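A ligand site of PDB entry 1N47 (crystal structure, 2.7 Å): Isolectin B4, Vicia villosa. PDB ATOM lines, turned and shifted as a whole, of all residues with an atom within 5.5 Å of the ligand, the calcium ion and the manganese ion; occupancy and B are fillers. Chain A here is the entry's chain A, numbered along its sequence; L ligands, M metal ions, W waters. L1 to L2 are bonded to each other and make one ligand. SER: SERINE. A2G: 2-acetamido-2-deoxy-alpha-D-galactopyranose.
The side-chain hydroxyl (OH) of Tyr 127 sits at hydrogen-bond distance from a nitrogen (N) of SER L1 (3.2 Å). The side-chain amide nitrogen (ND2) of Asn 129 sits at hydrogen-bond distance from an oxygen (O3) of A2G L2. The side-chain carboxylate (OD1) of Asp 85 is in hydrogen-bond range of an oxygen (O3) of A2G L2 (2.7 Å). N of Gly 103 is in hydrogen-bond range of O3 of A2G L2 (3.2 Å). N of Leu 213 is in hydrogen-bond range of O4 of A2G L2. O6 of A2G L2 sits at hydrogen-bond distance from OD1 of Asn 214 (3.3 Å).
Within 4 Å of the manganese ion: Glu 123, Asp 125, Asp 132 and His 137.
The calcium ion is bound by OD1 of Asp 132, OD1 of Asp 125, water W1, O of Tyr 127, OD2 of Asp 125 and OD1 of Asn 129.
The manganese ion is bound by OD2 of Asp 125, water W2, OE2 of Glu 123, OD2 of Asp 132, water W3 and NE2 of His 137. The manganese ion has six donor atoms within binding distance.
Along chain A the residues within 4 Å of the calcium ion span positions 125 to 132. The nearest printed residue that does not touch the calcium ion is Trp 131 (4.4 Å).
Water W3 bridges the backbone carbonyl oxygen (O) of Ile 145 (2.5 Å) and the side-chain carboxylate (OE1) of Glu 123 (2.7 Å).
OD1 of Asp 141 lies close to OE1 of Glu 123 (2.5 Å). The backbone carbonyl oxygen (O) of Asp 85 is in hydrogen-bond range of the backbone NH (N) of Thr 126, 3.4 Å away. N of Gly 212 lies close to O of Val 217 (3.4 Å). The backbone NH (N) of Gly 212 sits at hydrogen-bond distance from the backbone carbonyl oxygen (O) of Ala 84, at 3.5 Å.
Gly 102 touches the ligand. CA of Gly 212 touches O4 of A2G L2, at 3.8 Å. Val 217 touches the ligand. Hydrophobic or aromatic side chains that line the ligand: Tyr 127, Leu 213 and Val 217. Of the 25 residues printed, 9 come within 4 Å of the ligand. Along chain A the residues within 4 Å of the ligand span positions 85 to 217.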
ATOM      1  N   ALA A  84     -27.635  -3.236 -27.228  1.00  0.00           N
ATOM      2  CA  ALA A  84     -27.622  -4.356 -26.251  1.00  0.00           C
ATOM      3  C   ALA A  84     -27.202  -5.634 -26.957  1.00  0.00           C
ATOM      4  O   ALA A  84     -27.270  -5.665 -28.184  1.00  0.00           O
ATOM      5  CB  ALA A  84     -28.983  -4.537 -25.618  1.00  0.00           C
ATOM      6  N   ASP A  85     -26.740  -6.673 -26.243  1.00  0.00           N
ATOM      7  CA  ASP A  85     -26.589  -6.660 -24.783  1.00  0.00           C
ATOM      8  C   ASP A  85     -25.130  -6.755 -24.315  1.00  0.00           C
ATOM      9  O   ASP A  85     -24.897  -6.681 -23.111  1.00  0.00           O
ATOM     10  CB  ASP A  85     -27.294  -7.865 -24.138  1.00  0.00           C
ATOM     11  CG  ASP A  85     -28.759  -7.607 -23.829  1.00  0.00           C
ATOM     12  OD1 ASP A  85     -29.079  -7.113 -22.712  1.00  0.00           O
ATOM     13  OD2 ASP A  85     -29.661  -7.914 -24.640  1.00  0.00           O
ATOM     14  N   ARG A 101     -30.879 -16.002 -23.522  1.00  0.00           N
ATOM     15  CA  ARG A 101     -30.390 -14.883 -24.301  1.00  0.00           C
ATOM     16  C   ARG A 101     -30.639 -13.566 -23.573  1.00  0.00           C
ATOM     17  O   ARG A 101     -30.799 -13.549 -22.353  1.00  0.00           O
ATOM     18  CB  ARG A 101     -30.965 -14.890 -25.722  1.00  0.00           C
ATOM     19  CG  ARG A 101     -32.393 -15.408 -25.861  1.00  0.00           C
ATOM     20  CD  ARG A 101     -32.762 -15.787 -27.324  1.00  0.00           C
ATOM     21  NE  ARG A 101     -32.297 -17.138 -27.672  1.00  0.00           N
ATOM     22  CZ  ARG A 101     -31.803 -17.517 -28.856  1.00  0.00           C
ATOM     23  NH1 ARG A 101     -31.685 -16.653 -29.863  1.00  0.00           N
ATOM     24  NH2 ARG A 101     -31.417 -18.776 -29.028  1.00  0.00           N
ATOM     25  N   GLY A 102     -30.628 -12.453 -24.320  1.00  0.00           N
ATOM     26  CA  GLY A 102     -30.826 -11.151 -23.711  1.00  0.00           C
ATOM     27  C   GLY A 102     -29.682 -10.770 -22.785  1.00  0.00           C
ATOM     28  O   GLY A 102     -28.506 -10.904 -23.136  1.00  0.00           O
ATOM     29  N   GLY A 103     -30.018 -10.345 -21.578  1.00  0.00           N
ATOM     30  CA  GLY A 103     -29.020  -9.894 -20.633  1.00  0.00           C
ATOM     31  C   GLY A 103     -28.174 -10.954 -19.949  1.00  0.00           C
ATOM     32  O   GLY A 103     -27.338 -10.628 -19.088  1.00  0.00           O
ATOM     33  N   PHE A 104     -28.386 -12.215 -20.296  1.00  0.00           N
ATOM     34  CA  PHE A 104     -27.590 -13.302 -19.718  1.00  0.00           C
ATOM     35  C   PHE A 104     -26.431 -13.680 -20.645  1.00  0.00           C
ATOM     36  O   PHE A 104     -25.622 -14.554 -20.347  1.00  0.00           O
ATOM     37  CB  PHE A 104     -28.457 -14.512 -19.404  1.00  0.00           C
ATOM     38  CG  PHE A 104     -29.601 -14.212 -18.493  1.00  0.00           C
ATOM     39  CD1 PHE A 104     -29.419 -14.178 -17.105  1.00  0.00           C
ATOM     40  CD2 PHE A 104     -30.854 -13.957 -19.008  1.00  0.00           C
ATOM     41  CE1 PHE A 104     -30.504 -13.883 -16.249  1.00  0.00           C
ATOM     42  CE2 PHE A 104     -31.932 -13.663 -18.165  1.00  0.00           C
ATOM     43  CZ  PHE A 104     -31.764 -13.623 -16.794  1.00  0.00           C
ATOM     44  N   GLU A 123     -17.000  -9.762 -19.002  1.00  0.00           N
ATOM     45  CA  GLU A 123     -17.970  -9.204 -19.922  1.00  0.00           C
ATOM     46  C   GLU A 123     -17.684  -7.765 -20.217  1.00  0.00           C
ATOM     47  O   GLU A 123     -17.107  -7.066 -19.420  1.00  0.00           O
ATOM     48  CB  GLU A 123     -19.389  -9.262 -19.324  1.00  0.00           C
ATOM     49  CG  GLU A 123     -19.465  -8.948 -17.817  1.00  0.00           C
ATOM     50  CD  GLU A 123     -20.894  -8.690 -17.297  1.00  0.00           C
ATOM     51  OE1 GLU A 123     -21.628  -9.651 -16.982  1.00  0.00           O
ATOM     52  OE2 GLU A 123     -21.296  -7.505 -17.186  1.00  0.00           O
ATOM     53  N   ASP A 125     -20.300  -5.179 -20.994  1.00  0.00           N
ATOM     54  CA  ASP A 125     -21.757  -5.060 -20.873  1.00  0.00           C
ATOM     55  C   ASP A 125     -22.329  -3.739 -21.403  1.00  0.00           C
ATOM     56  O   ASP A 125     -21.977  -2.657 -20.898  1.00  0.00           O
ATOM     57  CB  ASP A 125     -22.062  -5.213 -19.377  1.00  0.00           C
ATOM     58  CG  ASP A 125     -23.470  -5.654 -19.097  1.00  0.00           C
ATOM     59  OD1 ASP A 125     -24.331  -5.451 -19.979  1.00  0.00           O
ATOM     60  OD2 ASP A 125     -23.809  -6.197 -18.016  1.00  0.00           O
ATOM     61  N   THR A 126     -23.214  -3.789 -22.408  1.00  0.00           N
ATOM     62  CA  THR A 126     -23.720  -2.552 -23.015  1.00  0.00           C
ATOM     63  C   THR A 126     -25.155  -2.128 -22.679  1.00  0.00           C
ATOM     64  O   THR A 126     -25.670  -1.175 -23.277  1.00  0.00           O
ATOM     65  CB  THR A 126     -23.583  -2.599 -24.539  1.00  0.00           C
ATOM     66  OG1 THR A 126     -24.275  -3.743 -25.037  1.00  0.00           O
ATOM     67  CG2 THR A 126     -22.132  -2.826 -24.963  1.00  0.00           C
ATOM     68  N   TYR A 127     -25.807  -2.805 -21.724  1.00  0.00           N
ATOM     69  CA  TYR A 127     -27.182  -2.435 -21.384  1.00  0.00           C
ATOM     70  C   TYR A 127     -27.486  -2.724 -19.931  1.00  0.00           C
ATOM     71  O   TYR A 127     -27.306  -3.842 -19.457  1.00  0.00           O
ATOM     72  CB  TYR A 127     -28.182  -3.161 -22.292  1.00  0.00           C
ATOM     73  CG  TYR A 127     -29.634  -2.964 -21.901  1.00  0.00           C
ATOM     74  CD1 TYR A 127     -30.183  -3.653 -20.825  1.00  0.00           C
ATOM     75  CD2 TYR A 127     -30.447  -2.072 -22.599  1.00  0.00           C
ATOM     76  CE1 TYR A 127     -31.496  -3.477 -20.466  1.00  0.00           C
ATOM     77  CE2 TYR A 127     -31.761  -1.882 -22.241  1.00  0.00           C
ATOM     78  CZ  TYR A 127     -32.293  -2.599 -21.170  1.00  0.00           C
ATOM     79  OH  TYR A 127     -33.618  -2.416 -20.794  1.00  0.00           O
ATOM     80  N   SER A 128     -27.968  -1.711 -19.207  1.00  0.00           N
ATOM     81  CA  SER A 128     -28.182  -1.898 -17.798  1.00  0.00           C
ATOM     82  C   SER A 128     -29.443  -2.662 -17.489  1.00  0.00           C
ATOM     83  O   SER A 128     -30.543  -2.188 -17.802  1.00  0.00           O
ATOM     84  CB  SER A 128     -28.211  -0.555 -17.068  1.00  0.00           C
ATOM     85  OG  SER A 128     -27.073   0.217 -17.369  1.00  0.00           O
ATOM     86  N   ASN A 129     -29.256  -3.826 -16.886  1.00  0.00           N
ATOM     87  CA  ASN A 129     -30.318  -4.673 -16.373  1.00  0.00           C
ATOM     88  C   ASN A 129     -30.457  -4.371 -14.898  1.00  0.00           C
ATOM     89  O   ASN A 129     -29.730  -3.536 -14.381  1.00  0.00           O
ATOM     90  CB  ASN A 129     -29.959  -6.158 -16.513  1.00  0.00           C
ATOM     91  CG  ASN A 129     -29.973  -6.637 -17.950  1.00  0.00           C
ATOM     92  OD1 ASN A 129     -28.922  -6.821 -18.569  1.00  0.00           O
ATOM     93  ND2 ASN A 129     -31.165  -6.854 -18.490  1.00  0.00           N
ATOM     94  N   ALA A 130     -31.329  -5.096 -14.210  1.00  0.00           N
ATOM     95  CA  ALA A 130     -31.636  -4.821 -12.821  1.00  0.00           C
ATOM     96  C   ALA A 130     -30.459  -5.091 -11.929  1.00  0.00           C
ATOM     97  O   ALA A 130     -30.314  -4.452 -10.899  1.00  0.00           O
ATOM     98  CB  ALA A 130     -32.871  -5.629 -12.355  1.00  0.00           C
ATOM     99  N   TRP A 131     -29.633  -6.054 -12.318  1.00  0.00           N
ATOM    100  CA  TRP A 131     -28.481  -6.476 -11.501  1.00  0.00           C
ATOM    101  C   TRP A 131     -27.211  -5.647 -11.812  1.00  0.00           C
ATOM    102  O   TRP A 131     -26.167  -5.811 -11.158  1.00  0.00           O
ATOM    103  CB  TRP A 131     -28.211  -7.975 -11.703  1.00  0.00           C
ATOM    104  CG  TRP A 131     -28.154  -8.345 -13.155  1.00  0.00           C
ATOM    105  CD1 TRP A 131     -27.128  -8.098 -14.034  1.00  0.00           C
ATOM    106  CD2 TRP A 131     -29.184  -8.970 -13.930  1.00  0.00           C
ATOM    107  NE1 TRP A 131     -27.459  -8.533 -15.284  1.00  0.00           N
ATOM    108  CE2 TRP A 131     -28.721  -9.086 -15.248  1.00  0.00           C
ATOM    109  CE3 TRP A 131     -30.482  -9.446 -13.633  1.00  0.00           C
ATOM    110  CZ2 TRP A 131     -29.476  -9.659 -16.269  1.00  0.00           C
ATOM    111  CZ3 TRP A 131     -31.223 -10.012 -14.638  1.00  0.00           C
ATOM    112  CH2 TRP A 131     -30.727 -10.125 -15.934  1.00  0.00           C
ATOM    113  N   ASP A 132     -27.322  -4.752 -12.777  1.00  0.00           N
ATOM    114  CA  ASP A 132     -26.196  -3.956 -13.234  1.00  0.00           C
ATOM    115  C   ASP A 132     -26.146  -2.535 -12.679  1.00  0.00           C
ATOM    116  O   ASP A 132     -27.118  -2.036 -12.093  1.00  0.00           O
ATOM    117  CB  ASP A 132     -26.255  -3.859 -14.761  1.00  0.00           C
ATOM    118  CG  ASP A 132     -25.738  -5.103 -15.457  1.00  0.00           C
ATOM    119  OD1 ASP A 132     -25.988  -5.257 -16.681  1.00  0.00           O
ATOM    120  OD2 ASP A 132     -25.067  -5.984 -14.855  1.00  0.00           O
ATOM    121  N   PRO A 133     -24.987  -1.907 -12.845  1.00  0.00           N
ATOM    122  CA  PRO A 133     -24.818  -0.473 -12.564  1.00  0.00           C
ATOM    123  C   PRO A 133     -25.457   0.289 -13.704  1.00  0.00           C
ATOM    124  O   PRO A 133     -25.727  -0.315 -14.744  1.00  0.00           O
ATOM    125  CB  PRO A 133     -23.309  -0.276 -12.635  1.00  0.00           C
ATOM    126  CG  PRO A 133     -22.761  -1.631 -12.542  1.00  0.00           C
ATOM    127  CD  PRO A 133     -23.733  -2.521 -13.284  1.00  0.00           C
ATOM    128  N   HIS A 137     -20.136  -1.058 -18.840  1.00  0.00           N
ATOM    129  CA  HIS A 137     -19.080  -1.491 -17.941  1.00  0.00           C
ATOM    130  C   HIS A 137     -18.453  -2.818 -18.288  1.00  0.00           C
ATOM    131  O   HIS A 137     -19.025  -3.642 -19.001  1.00  0.00           O
ATOM    132  CB  HIS A 137     -19.674  -1.671 -16.565  1.00  0.00           C
ATOM    133  CG  HIS A 137     -20.790  -2.655 -16.542  1.00  0.00           C
ATOM    134  ND1 HIS A 137     -22.047  -2.349 -17.001  1.00  0.00           N
ATOM    135  CD2 HIS A 137     -20.840  -3.951 -16.151  1.00  0.00           C
ATOM    136  CE1 HIS A 137     -22.837  -3.404 -16.870  1.00  0.00           C
ATOM    137  NE2 HIS A 137     -22.129  -4.391 -16.354  1.00  0.00           N
ATOM    138  N   ASP A 141     -17.484 -11.908 -14.076  1.00  0.00           N
ATOM    139  CA  ASP A 141     -18.493 -12.846 -13.639  1.00  0.00           C
ATOM    140  C   ASP A 141     -17.900 -14.152 -13.145  1.00  0.00           C
ATOM    141  O   ASP A 141     -17.209 -14.813 -13.888  1.00  0.00           O
ATOM    142  CB  ASP A 141     -19.418 -13.115 -14.820  1.00  0.00           C
ATOM    143  CG  ASP A 141     -20.206 -11.889 -15.235  1.00  0.00           C
ATOM    144  OD1 ASP A 141     -20.742 -11.865 -16.358  1.00  0.00           O
ATOM    145  OD2 ASP A 141     -20.337 -10.885 -14.528  1.00  0.00           O
ATOM    146  N   ILE A 145     -24.438 -13.864 -13.361  1.00  0.00           N
ATOM    147  CA  ILE A 145     -24.500 -12.650 -14.194  1.00  0.00           C
ATOM    148  C   ILE A 145     -24.261 -11.367 -13.375  1.00  0.00           C
ATOM    149  O   ILE A 145     -24.025 -10.299 -13.927  1.00  0.00           O
ATOM    150  CB  ILE A 145     -25.881 -12.613 -14.897  1.00  0.00           C
ATOM    151  CG1 ILE A 145     -25.926 -11.576 -16.003  1.00  0.00           C
ATOM    152  CG2 ILE A 145     -27.003 -12.373 -13.898  1.00  0.00           C
ATOM    153  CD1 ILE A 145     -25.018 -11.910 -17.140  1.00  0.00           C
ATOM    154  N   SER A 147     -21.943  -9.493 -11.571  1.00  0.00           N
ATOM    155  CA  SER A 147     -20.481  -9.436 -11.472  1.00  0.00           C
ATOM    156  C   SER A 147     -19.953  -9.268 -10.071  1.00  0.00           C
ATOM    157  O   SER A 147     -20.537  -8.606  -9.254  1.00  0.00           O
ATOM    158  CB  SER A 147     -19.924  -8.358 -12.358  1.00  0.00           C
ATOM    159  OG  SER A 147     -20.373  -8.582 -13.671  1.00  0.00           O
ATOM    160  N   THR A 211     -27.960  -9.991 -28.746  1.00  0.00           N
ATOM    161  CA  THR A 211     -28.576  -8.703 -29.064  1.00  0.00           C
ATOM    162  C   THR A 211     -29.753  -8.469 -28.148  1.00  0.00           C
ATOM    163  O   THR A 211     -30.112  -9.318 -27.363  1.00  0.00           O
ATOM    164  CB  THR A 211     -29.072  -8.649 -30.468  1.00  0.00           C
ATOM    165  OG1 THR A 211     -29.657  -9.910 -30.819  1.00  0.00           O
ATOM    166  CG2 THR A 211     -27.908  -8.482 -31.430  1.00  0.00           C
ATOM    167  N   GLY A 212     -30.363  -7.295 -28.272  1.00  0.00           N
ATOM    168  CA  GLY A 212     -31.512  -6.934 -27.455  1.00  0.00           C
ATOM    169  C   GLY A 212     -32.782  -7.723 -27.741  1.00  0.00           C
ATOM    170  O   GLY A 212     -33.036  -8.143 -28.869  1.00  0.00           O
ATOM    171  N   LEU A 213     -33.556  -7.929 -26.682  1.00  0.00           N
ATOM    172  CA  LEU A 213     -34.835  -8.628 -26.773  1.00  0.00           C
ATOM    173  C   LEU A 213     -35.912  -7.773 -27.458  1.00  0.00           C
ATOM    174  O   LEU A 213     -36.926  -8.294 -27.850  1.00  0.00           O
ATOM    175  CB  LEU A 213     -35.341  -9.058 -25.395  1.00  0.00           C
ATOM    176  CG  LEU A 213     -34.642 -10.248 -24.744  1.00  0.00           C
ATOM    177  CD1 LEU A 213     -35.399 -10.782 -23.520  1.00  0.00           C
ATOM    178  CD2 LEU A 213     -34.452 -11.356 -25.747  1.00  0.00           C
ATOM    179  N   ASN A 214     -35.689  -6.474 -27.594  1.00  0.00           N
ATOM    180  CA  ASN A 214     -36.700  -5.635 -28.231  1.00  0.00           C
ATOM    181  C   ASN A 214     -36.282  -5.038 -29.562  1.00  0.00           C
ATOM    182  O   ASN A 214     -35.127  -4.709 -29.781  1.00  0.00           O
ATOM    183  CB  ASN A 214     -37.174  -4.531 -27.302  1.00  0.00           C
ATOM    184  CG  ASN A 214     -38.111  -5.045 -26.246  1.00  0.00           C
ATOM    185  OD1 ASN A 214     -37.730  -5.190 -25.086  1.00  0.00           O
ATOM    186  ND2 ASN A 214     -39.338  -5.345 -26.642  1.00  0.00           N
ATOM    187  N   VAL A 217     -33.131  -2.347 -30.466  1.00  0.00           N
ATOM    188  CA  VAL A 217     -32.309  -2.127 -29.282  1.00  0.00           C
ATOM    189  C   VAL A 217     -31.101  -3.052 -29.380  1.00  0.00           C
ATOM    190  O   VAL A 217     -30.869  -3.902 -28.523  1.00  0.00           O
ATOM    191  CB  VAL A 217     -33.184  -2.391 -28.070  1.00  0.00           C
ATOM    192  CG1 VAL A 217     -32.386  -2.382 -26.803  1.00  0.00           C
ATOM    193  CG2 VAL A 217     -34.294  -1.341 -28.053  1.00  0.00           C
HETATM  194  N   SER L   1     -35.933  -3.471 -18.803  1.00  0.00           N
HETATM  195  CA  SER L   1     -36.449  -4.836 -18.929  1.00  0.00           C
HETATM  196  C   SER L   1     -35.686  -5.816 -18.023  1.00  0.00           C
HETATM  197  O   SER L   1     -34.563  -5.536 -17.607  1.00  0.00           O
HETATM  198  CB  SER L   1     -36.397  -5.277 -20.401  1.00  0.00           C
HETATM  199  OG  SER L   1     -35.108  -5.752 -20.760  1.00  0.00           O
HETATM  200  OXT SER L   1     -36.187  -6.884 -17.690  1.00  0.00           O
HETATM  201  O5  A2G L   2     -34.959  -6.252 -23.035  1.00  0.00           O
HETATM  202  C1  A2G L   2     -35.005  -6.800 -21.724  1.00  0.00           C
HETATM  203  C2  A2G L   2     -33.743  -7.612 -21.423  1.00  0.00           C
HETATM  204  N2  A2G L   2     -33.904  -8.138 -20.100  1.00  0.00           N
HETATM  205  C3  A2G L   2     -32.537  -6.711 -21.525  1.00  0.00           C
HETATM  206  O3  A2G L   2     -31.381  -7.503 -21.304  1.00  0.00           O
HETATM  207  C4  A2G L   2     -32.490  -6.179 -22.934  1.00  0.00           C
HETATM  208  O4  A2G L   2     -32.331  -7.299 -23.807  1.00  0.00           O
HETATM  209  C5  A2G L   2     -33.790  -5.470 -23.293  1.00  0.00           C
HETATM  210  C6  A2G L   2     -33.777  -5.141 -24.774  1.00  0.00           C
HETATM  211  O6  A2G L   2     -34.657  -4.035 -25.005  1.00  0.00           O
HETATM  212  C7  A2G L   2     -33.674  -9.415 -19.861  1.00  0.00           C
HETATM  213  O7  A2G L   2     -33.296 -10.148 -20.755  1.00  0.00           O
HETATM  214  C8  A2G L   2     -33.901  -9.893 -18.454  1.00  0.00           C
HETATM  215 CA    CA M   1     -26.323  -6.090 -18.740  1.00  0.00          CA
HETATM  216 MN    MN M   2     -23.219  -6.617 -16.225  1.00  0.00          MN
HETATM  217  O   HOH W   1     -26.562  -6.651 -21.161  1.00  0.00           O
HETATM  218  O   HOH W   2     -22.164  -6.784 -14.396  1.00  0.00           O
HETATM  219  O   HOH W   3     -24.021  -8.910 -16.020  1.00  0.00           O
